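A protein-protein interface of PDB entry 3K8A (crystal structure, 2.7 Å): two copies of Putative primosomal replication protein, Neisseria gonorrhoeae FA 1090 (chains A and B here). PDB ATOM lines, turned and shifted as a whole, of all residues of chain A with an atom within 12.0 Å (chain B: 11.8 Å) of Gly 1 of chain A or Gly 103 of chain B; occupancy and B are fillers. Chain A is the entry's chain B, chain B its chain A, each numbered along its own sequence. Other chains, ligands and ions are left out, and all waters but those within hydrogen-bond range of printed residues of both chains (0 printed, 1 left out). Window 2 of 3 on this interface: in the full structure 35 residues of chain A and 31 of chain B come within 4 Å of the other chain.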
ATOM      1  N   GLY A   1       0.069  29.640  14.621  1.00  0.00           N
ATOM      2  CA  GLY A   1       0.894  28.402  14.733  1.00  0.00           C
ATOM      3  C   GLY A   1       0.579  27.581  15.974  1.00  0.00           C
ATOM      4  O   GLY A   1       0.561  28.104  17.087  1.00  0.00           O
ATOM      5  N   SER A   2       0.300  26.292  15.769  1.00  0.00           N
ATOM      6  CA  SER A   2       0.196  25.303  16.852  1.00  0.00           C
ATOM      7  C   SER A   2      -0.365  23.990  16.268  1.00  0.00           C
ATOM      8  O   SER A   2      -1.495  23.952  15.763  1.00  0.00           O
ATOM      9  CB  SER A   2      -0.587  25.840  18.070  1.00  0.00           C
ATOM     10  OG  SER A   2      -1.886  25.286  18.173  1.00  0.00           O
ATOM     11  N   HIS A   3       0.457  22.936  16.306  1.00  0.00           N
ATOM     12  CA  HIS A   3       0.064  21.584  15.871  1.00  0.00           C
ATOM     13  C   HIS A   3      -0.455  20.797  17.068  1.00  0.00           C
ATOM     14  O   HIS A   3      -0.919  19.673  16.922  1.00  0.00           O
ATOM     15  CB  HIS A   3       1.236  20.824  15.228  1.00  0.00           C
ATOM     16  CG  HIS A   3       2.524  20.936  15.992  1.00  0.00           C
ATOM     17  ND1 HIS A   3       3.738  21.168  15.377  1.00  0.00           N
ATOM     18  CD2 HIS A   3       2.783  20.863  17.322  1.00  0.00           C
ATOM     19  CE1 HIS A   3       4.689  21.225  16.294  1.00  0.00           C
ATOM     20  NE2 HIS A   3       4.136  21.045  17.482  1.00  0.00           N
ATOM     21  N   MET A   4      -0.348  21.383  18.258  1.00  0.00           N
ATOM     22  CA  MET A   4      -0.996  20.824  19.435  1.00  0.00           C
ATOM     23  C   MET A   4      -2.444  20.496  19.028  1.00  0.00           C
ATOM     24  O   MET A   4      -2.934  20.984  17.997  1.00  0.00           O
ATOM     25  CB  MET A   4      -0.971  21.846  20.591  1.00  0.00           C
ATOM     26  CG  MET A   4      -2.200  22.809  20.640  1.00  0.00           C
ATOM     27  SD  MET A   4      -1.876  24.593  20.879  1.00  0.00           S
ATOM     28  CE  MET A   4      -3.463  25.177  21.516  1.00  0.00           C
ATOM     29  N   GLY A   5      -3.123  19.668  19.824  1.00  0.00           N
ATOM     30  CA  GLY A   5      -4.551  19.424  19.624  1.00  0.00           C
ATOM     31  C   GLY A   5      -5.325  20.633  20.112  1.00  0.00           C
ATOM     32  O   GLY A   5      -4.766  21.734  20.261  1.00  0.00           O
ATOM     33  N   PHE A   6      -6.618  20.442  20.348  1.00  0.00           N
ATOM     34  CA  PHE A   6      -7.402  21.465  20.996  1.00  0.00           C
ATOM     35  C   PHE A   6      -7.174  21.285  22.513  1.00  0.00           C
ATOM     36  O   PHE A   6      -7.022  20.163  22.980  1.00  0.00           O
ATOM     37  CB  PHE A   6      -8.874  21.356  20.567  1.00  0.00           C
ATOM     38  CG  PHE A   6      -9.128  21.786  19.129  1.00  0.00           C
ATOM     39  CD1 PHE A   6      -9.157  20.860  18.102  1.00  0.00           C
ATOM     40  CD2 PHE A   6      -9.323  23.123  18.816  1.00  0.00           C
ATOM     41  CE1 PHE A   6      -9.365  21.249  16.811  1.00  0.00           C
ATOM     42  CE2 PHE A   6      -9.533  23.527  17.512  1.00  0.00           C
ATOM     43  CZ  PHE A   6      -9.556  22.588  16.500  1.00  0.00           C
ATOM     44  N   THR A   7      -7.111  22.382  23.261  1.00  0.00           N
ATOM     45  CA  THR A   7      -6.638  22.326  24.637  1.00  0.00           C
ATOM     46  C   THR A   7      -7.561  21.530  25.550  1.00  0.00           C
ATOM     47  O   THR A   7      -8.719  21.867  25.754  1.00  0.00           O
ATOM     48  CB  THR A   7      -6.371  23.746  25.239  1.00  0.00           C
ATOM     49  OG1 THR A   7      -5.808  24.588  24.237  1.00  0.00           O
ATOM     50  CG2 THR A   7      -5.390  23.667  26.374  1.00  0.00           C
ATOM     51  N   ASN A   8      -7.046  20.463  26.115  1.00  0.00           N
ATOM     52  CA  ASN A   8      -7.804  19.755  27.122  1.00  0.00           C
ATOM     53  C   ASN A   8      -6.905  19.461  28.341  1.00  0.00           C
ATOM     54  O   ASN A   8      -6.257  18.419  28.398  1.00  0.00           O
ATOM     55  CB  ASN A   8      -8.395  18.487  26.515  1.00  0.00           C
ATOM     56  CG  ASN A   8      -9.469  17.847  27.403  1.00  0.00           C
ATOM     57  OD1 ASN A   8      -9.387  17.868  28.644  1.00  0.00           O
ATOM     58  ND2 ASN A   8     -10.468  17.253  26.768  1.00  0.00           N
ATOM     59  N   LEU A   9      -6.831  20.400  29.278  1.00  0.00           N
ATOM     60  CA  LEU A   9      -5.933  20.270  30.437  1.00  0.00           C
ATOM     61  C   LEU A   9      -6.606  20.400  31.793  1.00  0.00           C
ATOM     62  O   LEU A   9      -7.033  21.487  32.167  1.00  0.00           O
ATOM     63  CB  LEU A   9      -4.861  21.337  30.390  1.00  0.00           C
ATOM     64  CG  LEU A   9      -3.526  21.049  29.754  1.00  0.00           C
ATOM     65  CD1 LEU A   9      -2.965  22.357  29.186  1.00  0.00           C
ATOM     66  CD2 LEU A   9      -2.621  20.432  30.834  1.00  0.00           C
ATOM     67  N   SER B  11      -8.164  23.931  31.631  1.00  0.00           N
ATOM     68  CA  SER B  11      -8.190  24.747  30.381  1.00  0.00           C
ATOM     69  C   SER B  11      -8.740  23.844  29.326  1.00  0.00           C
ATOM     70  O   SER B  11      -8.196  22.747  29.090  1.00  0.00           O
ATOM     71  CB  SER B  11      -6.805  25.179  29.883  1.00  0.00           C
ATOM     72  OG  SER B  11      -6.005  25.709  30.926  1.00  0.00           O
ATOM     73  N   LEU B  12      -9.804  24.308  28.682  1.00  0.00           N
ATOM     74  CA  LEU B  12     -10.472  23.545  27.641  1.00  0.00           C
ATOM     75  C   LEU B  12     -10.807  24.459  26.497  1.00  0.00           C
ATOM     76  O   LEU B  12     -11.293  25.569  26.700  1.00  0.00           O
ATOM     77  CB  LEU B  12     -11.764  22.955  28.197  1.00  0.00           C
ATOM     78  CG  LEU B  12     -12.489  21.933  27.326  1.00  0.00           C
ATOM     79  CD1 LEU B  12     -11.752  20.557  27.303  1.00  0.00           C
ATOM     80  CD2 LEU B  12     -13.945  21.788  27.791  1.00  0.00           C
ATOM     81  N   ALA B  13     -10.532  23.992  25.288  1.00  0.00           N
ATOM     82  CA  ALA B  13     -10.925  24.681  24.071  1.00  0.00           C
ATOM     83  C   ALA B  13     -12.139  23.915  23.639  1.00  0.00           C
ATOM     84  O   ALA B  13     -12.110  22.692  23.681  1.00  0.00           O
ATOM     85  CB  ALA B  13      -9.866  24.558  23.062  1.00  0.00           C
ATOM     86  N   ALA B  14     -13.210  24.607  23.244  1.00  0.00           N
ATOM     87  CA  ALA B  14     -14.503  23.950  23.027  1.00  0.00           C
ATOM     88  C   ALA B  14     -15.556  24.870  22.414  1.00  0.00           C
ATOM     89  O   ALA B  14     -15.565  26.062  22.684  1.00  0.00           O
ATOM     90  CB  ALA B  14     -15.008  23.385  24.336  1.00  0.00           C
ATOM     91  N   TRP B  67     -20.698  37.298  26.543  1.00  0.00           N
ATOM     92  CA  TRP B  67     -20.640  35.987  25.900  1.00  0.00           C
ATOM     93  C   TRP B  67     -21.992  35.312  25.679  1.00  0.00           C
ATOM     94  O   TRP B  67     -22.056  34.261  25.050  1.00  0.00           O
ATOM     95  CB  TRP B  67     -19.670  35.047  26.654  1.00  0.00           C
ATOM     96  CG  TRP B  67     -18.235  35.347  26.318  1.00  0.00           C
ATOM     97  CD1 TRP B  67     -17.430  36.289  26.898  1.00  0.00           C
ATOM     98  CD2 TRP B  67     -17.465  34.754  25.273  1.00  0.00           C
ATOM     99  NE1 TRP B  67     -16.201  36.303  26.291  1.00  0.00           N
ATOM    100  CE2 TRP B  67     -16.193  35.369  25.290  1.00  0.00           C
ATOM    101  CE3 TRP B  67     -17.722  33.748  24.335  1.00  0.00           C
ATOM    102  CZ2 TRP B  67     -15.179  35.008  24.412  1.00  0.00           C
ATOM    103  CZ3 TRP B  67     -16.722  33.393  23.467  1.00  0.00           C
ATOM    104  CH2 TRP B  67     -15.459  34.020  23.510  1.00  0.00           C
ATOM    105  N   CYS B  74     -16.222  29.026  19.039  1.00  0.00           N
ATOM    106  CA  CYS B  74     -15.186  28.206  19.654  1.00  0.00           C
ATOM    107  C   CYS B  74     -14.332  29.005  20.647  1.00  0.00           C
ATOM    108  O   CYS B  74     -13.735  30.014  20.299  1.00  0.00           O
ATOM    109  CB  CYS B  74     -14.295  27.587  18.572  1.00  0.00           C
ATOM    110  SG  CYS B  74     -13.018  26.523  19.264  1.00  0.00           S
ATOM    111  N   ALA B  75     -14.253  28.549  21.886  1.00  0.00           N
ATOM    112  CA  ALA B  75     -13.592  29.339  22.917  1.00  0.00           C
ATOM    113  C   ALA B  75     -12.498  28.567  23.671  1.00  0.00           C
ATOM    114  O   ALA B  75     -12.584  27.353  23.806  1.00  0.00           O
ATOM    115  CB  ALA B  75     -14.630  29.860  23.890  1.00  0.00           C
ATOM    116  N   THR B  76     -11.462  29.256  24.145  1.00  0.00           N
ATOM    117  CA  THR B  76     -10.627  28.683  25.186  1.00  0.00           C
ATOM    118  C   THR B  76     -11.219  29.113  26.501  1.00  0.00           C
ATOM    119  O   THR B  76     -11.658  30.239  26.657  1.00  0.00           O
ATOM    120  CB  THR B  76      -9.185  29.187  25.183  1.00  0.00           C
ATOM    121  OG1 THR B  76      -8.649  29.118  23.860  1.00  0.00           O
ATOM    122  CG2 THR B  76      -8.335  28.329  26.141  1.00  0.00           C
ATOM    123  N   VAL B  77     -11.193  28.211  27.456  1.00  0.00           N
ATOM    124  CA  VAL B  77     -11.847  28.432  28.721  1.00  0.00           C
ATOM    125  C   VAL B  77     -10.918  27.968  29.824  1.00  0.00           C
ATOM    126  O   VAL B  77     -10.237  26.951  29.687  1.00  0.00           O
ATOM    127  CB  VAL B  77     -13.170  27.639  28.791  1.00  0.00           C
ATOM    128  CG1 VAL B  77     -13.724  27.695  30.170  1.00  0.00           C
ATOM    129  CG2 VAL B  77     -14.179  28.221  27.840  1.00  0.00           C
ATOM    130  N   ILE B  98     -12.565  33.426  29.769  1.00  0.00           N
ATOM    131  CA  ILE B  98     -13.011  32.847  28.503  1.00  0.00           C
ATOM    132  C   ILE B  98     -12.618  33.710  27.289  1.00  0.00           C
ATOM    133  O   ILE B  98     -13.149  34.793  27.101  1.00  0.00           O
ATOM    134  CB  ILE B  98     -14.543  32.577  28.548  1.00  0.00           C
ATOM    135  CG1 ILE B  98     -15.070  32.177  27.175  1.00  0.00           C
ATOM    136  CG2 ILE B  98     -15.301  33.800  29.055  1.00  0.00           C
ATOM    137  CD1 ILE B  98     -16.516  31.805  27.210  1.00  0.00           C
ATOM    138  N   LYS B  99     -11.672  33.229  26.480  1.00  0.00           N
ATOM    139  CA  LYS B  99     -11.175  33.967  25.317  1.00  0.00           C
ATOM    140  C   LYS B  99     -11.844  33.325  24.127  1.00  0.00           C
ATOM    141  O   LYS B  99     -12.451  32.288  24.274  1.00  0.00           O
ATOM    142  CB  LYS B  99      -9.657  33.782  25.175  1.00  0.00           C
ATOM    143  CG  LYS B  99      -8.838  34.099  26.408  1.00  0.00           C
ATOM    144  CD  LYS B  99      -8.446  35.573  26.374  1.00  0.00           C
ATOM    145  CE  LYS B  99      -8.283  36.194  27.762  1.00  0.00           C
ATOM    146  NZ  LYS B  99      -7.052  35.734  28.460  1.00  0.00           N
ATOM    147  N   GLU B 100     -11.725  33.923  22.946  1.00  0.00           N
ATOM    148  CA  GLU B 100     -11.999  33.204  21.697  1.00  0.00           C
ATOM    149  C   GLU B 100     -10.765  32.385  21.351  1.00  0.00           C
ATOM    150  O   GLU B 100      -9.674  32.940  21.270  1.00  0.00           O
ATOM    151  CB  GLU B 100     -12.238  34.169  20.537  1.00  0.00           C
ATOM    152  CG  GLU B 100     -13.615  34.757  20.453  1.00  0.00           C
ATOM    153  CD  GLU B 100     -13.596  36.107  19.755  1.00  0.00           C
ATOM    154  OE1 GLU B 100     -12.966  36.204  18.677  1.00  0.00           O
ATOM    155  OE2 GLU B 100     -14.191  37.077  20.285  1.00  0.00           O
ATOM    156  N   TYR B 101     -10.929  31.083  21.122  1.00  0.00           N
ATOM    157  CA  TYR B 101      -9.787  30.237  20.755  1.00  0.00           C
ATOM    158  C   TYR B 101      -8.998  30.781  19.574  1.00  0.00           C
ATOM    159  O   TYR B 101      -9.550  31.025  18.504  1.00  0.00           O
ATOM    160  CB  TYR B 101     -10.233  28.819  20.416  1.00  0.00           C
ATOM    161  CG  TYR B 101      -9.096  27.879  20.073  1.00  0.00           C
ATOM    162  CD1 TYR B 101      -8.351  27.282  21.072  1.00  0.00           C
ATOM    163  CD2 TYR B 101      -8.780  27.576  18.752  1.00  0.00           C
ATOM    164  CE1 TYR B 101      -7.312  26.407  20.784  1.00  0.00           C
ATOM    165  CE2 TYR B 101      -7.737  26.702  18.446  1.00  0.00           C
ATOM    166  CZ  TYR B 101      -7.007  26.118  19.477  1.00  0.00           C
ATOM    167  OH  TYR B 101      -5.965  25.250  19.225  1.00  0.00           O
ATOM    168  N   LYS B 102      -7.700  30.968  19.771  1.00  0.00           N
ATOM    169  CA  LYS B 102      -6.814  31.205  18.649  1.00  0.00           C
ATOM    170  C   LYS B 102      -5.575  30.321  18.771  1.00  0.00           C
ATOM    171  O   LYS B 102      -4.716  30.325  17.891  1.00  0.00           O
ATOM    172  CB  LYS B 102      -6.445  32.682  18.528  1.00  0.00           C
ATOM    173  CG  LYS B 102      -6.158  33.096  17.091  1.00  0.00           C
ATOM    174  CD  LYS B 102      -6.493  34.567  16.849  1.00  0.00           C
ATOM    175  CE  LYS B 102      -7.916  34.899  17.285  1.00  0.00           C
ATOM    176  NZ  LYS B 102      -8.275  36.295  16.917  1.00  0.00           N
ATOM    177  N   GLY B 103      -5.518  29.547  19.854  1.00  0.00           N
ATOM    178  CA  GLY B 103      -4.389  28.678  20.153  1.00  0.00           C
ATOM    179  C   GLY B 103      -3.371  28.608  19.030  1.00  0.00           C
ATOM    180  O   GLY B 103      -2.391  29.362  19.006  1.00  0.00           O
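Among the printed residues, merely in contact across the chains: Gly 1 of chain A with Gly 103 of chain B (3.7 Å), Ser 2 of chain A with Gly 103 of chain B (3.7 Å), Met 4 of chain A with Tyr 101 of chain B (3.4 Å), Met 4 of chain A with Gly 103 of chain B (3.9 Å), Gly 5 of chain A with Tyr 101 of chain B (3.9 Å), Phe 6 of chain A with Tyr 101 of chain B (3.8 Å), Thr 7 of chain A with Leu 12 of chain B (3.1 Å), Asn 8 of chain A with Ser 11 of chain B (3.6 Å) and Asn 8 of chain A with Leu 12 of chain B (3.5 Å).
Hydrophobic or aromatic side chains of chain A within 4 Å of the printed part of chain B: Met 4, Phe 6 and Leu 9.
Gly 1 of chain A touches just one residue of chain B: Gly 103.
Of chain B, only Gly 103 (3.7 Å) comes within 4 Å of Ser 2 of chain A.
Of the printed residues of chain B, Phe 6 of chain A touches Tyr 101.
Of the printed residues of chain B, Leu 9 of chain A touches Ser 11 (2.7 Å).
Of the printed residues of chain A, Ala 13 of chain B touches Thr 7.
Tyr 101 of chain B touches just these residues of chain A: Met 4 (3.4 Å), Gly 5 (3.9 Å) and Phe 6 (3.8 Å).
Gly 103 of chain B touches just these residues of chain A: Gly 1 (3.7 Å), Ser 2 (3.7 Å) and Met 4 (3.9 Å).
The nearest residue of chain B that does not touch Gly 1 of chain A is Lys 102 of chain B (5.8 Å).
The nearest residue of chain A that does not touch Gly 103 of chain B is Thr 7 of chain A (6.0 Å).
The backbone carbonyl oxygen (O) of Ser 11 of chain B is in hydrogen-bond range of the backbone NH (N) of Leu 9 of chain A, 2.7 Å away.
O of Thr 7 of chain A sits close to O of Ser 11 of chain B, at 3.5 Å.
The backbone carbonyl oxygen (O) of Thr 7 of chain A lies within hydrogen-bond range of the backbone NH (N) of Ala 13 of chain B (2.8 Å).
The backbone carbonyl oxygen (O) of Leu 12 of chain B sits at hydrogen-bond distance from the backbone NH (N) of Val 77 of chain B (2.7 Å).
The side-chain hydroxyl (OG) of Ser 2 of chain A lies within hydrogen-bond range of the side-chain sulfur (SD) of Met 4 of chain A, 2.8 Å away.
O of Cys 74 of chain B is in hydrogen-bond range of N of Tyr 101 of chain B (3.1 Å).
No position is printed for both chains.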
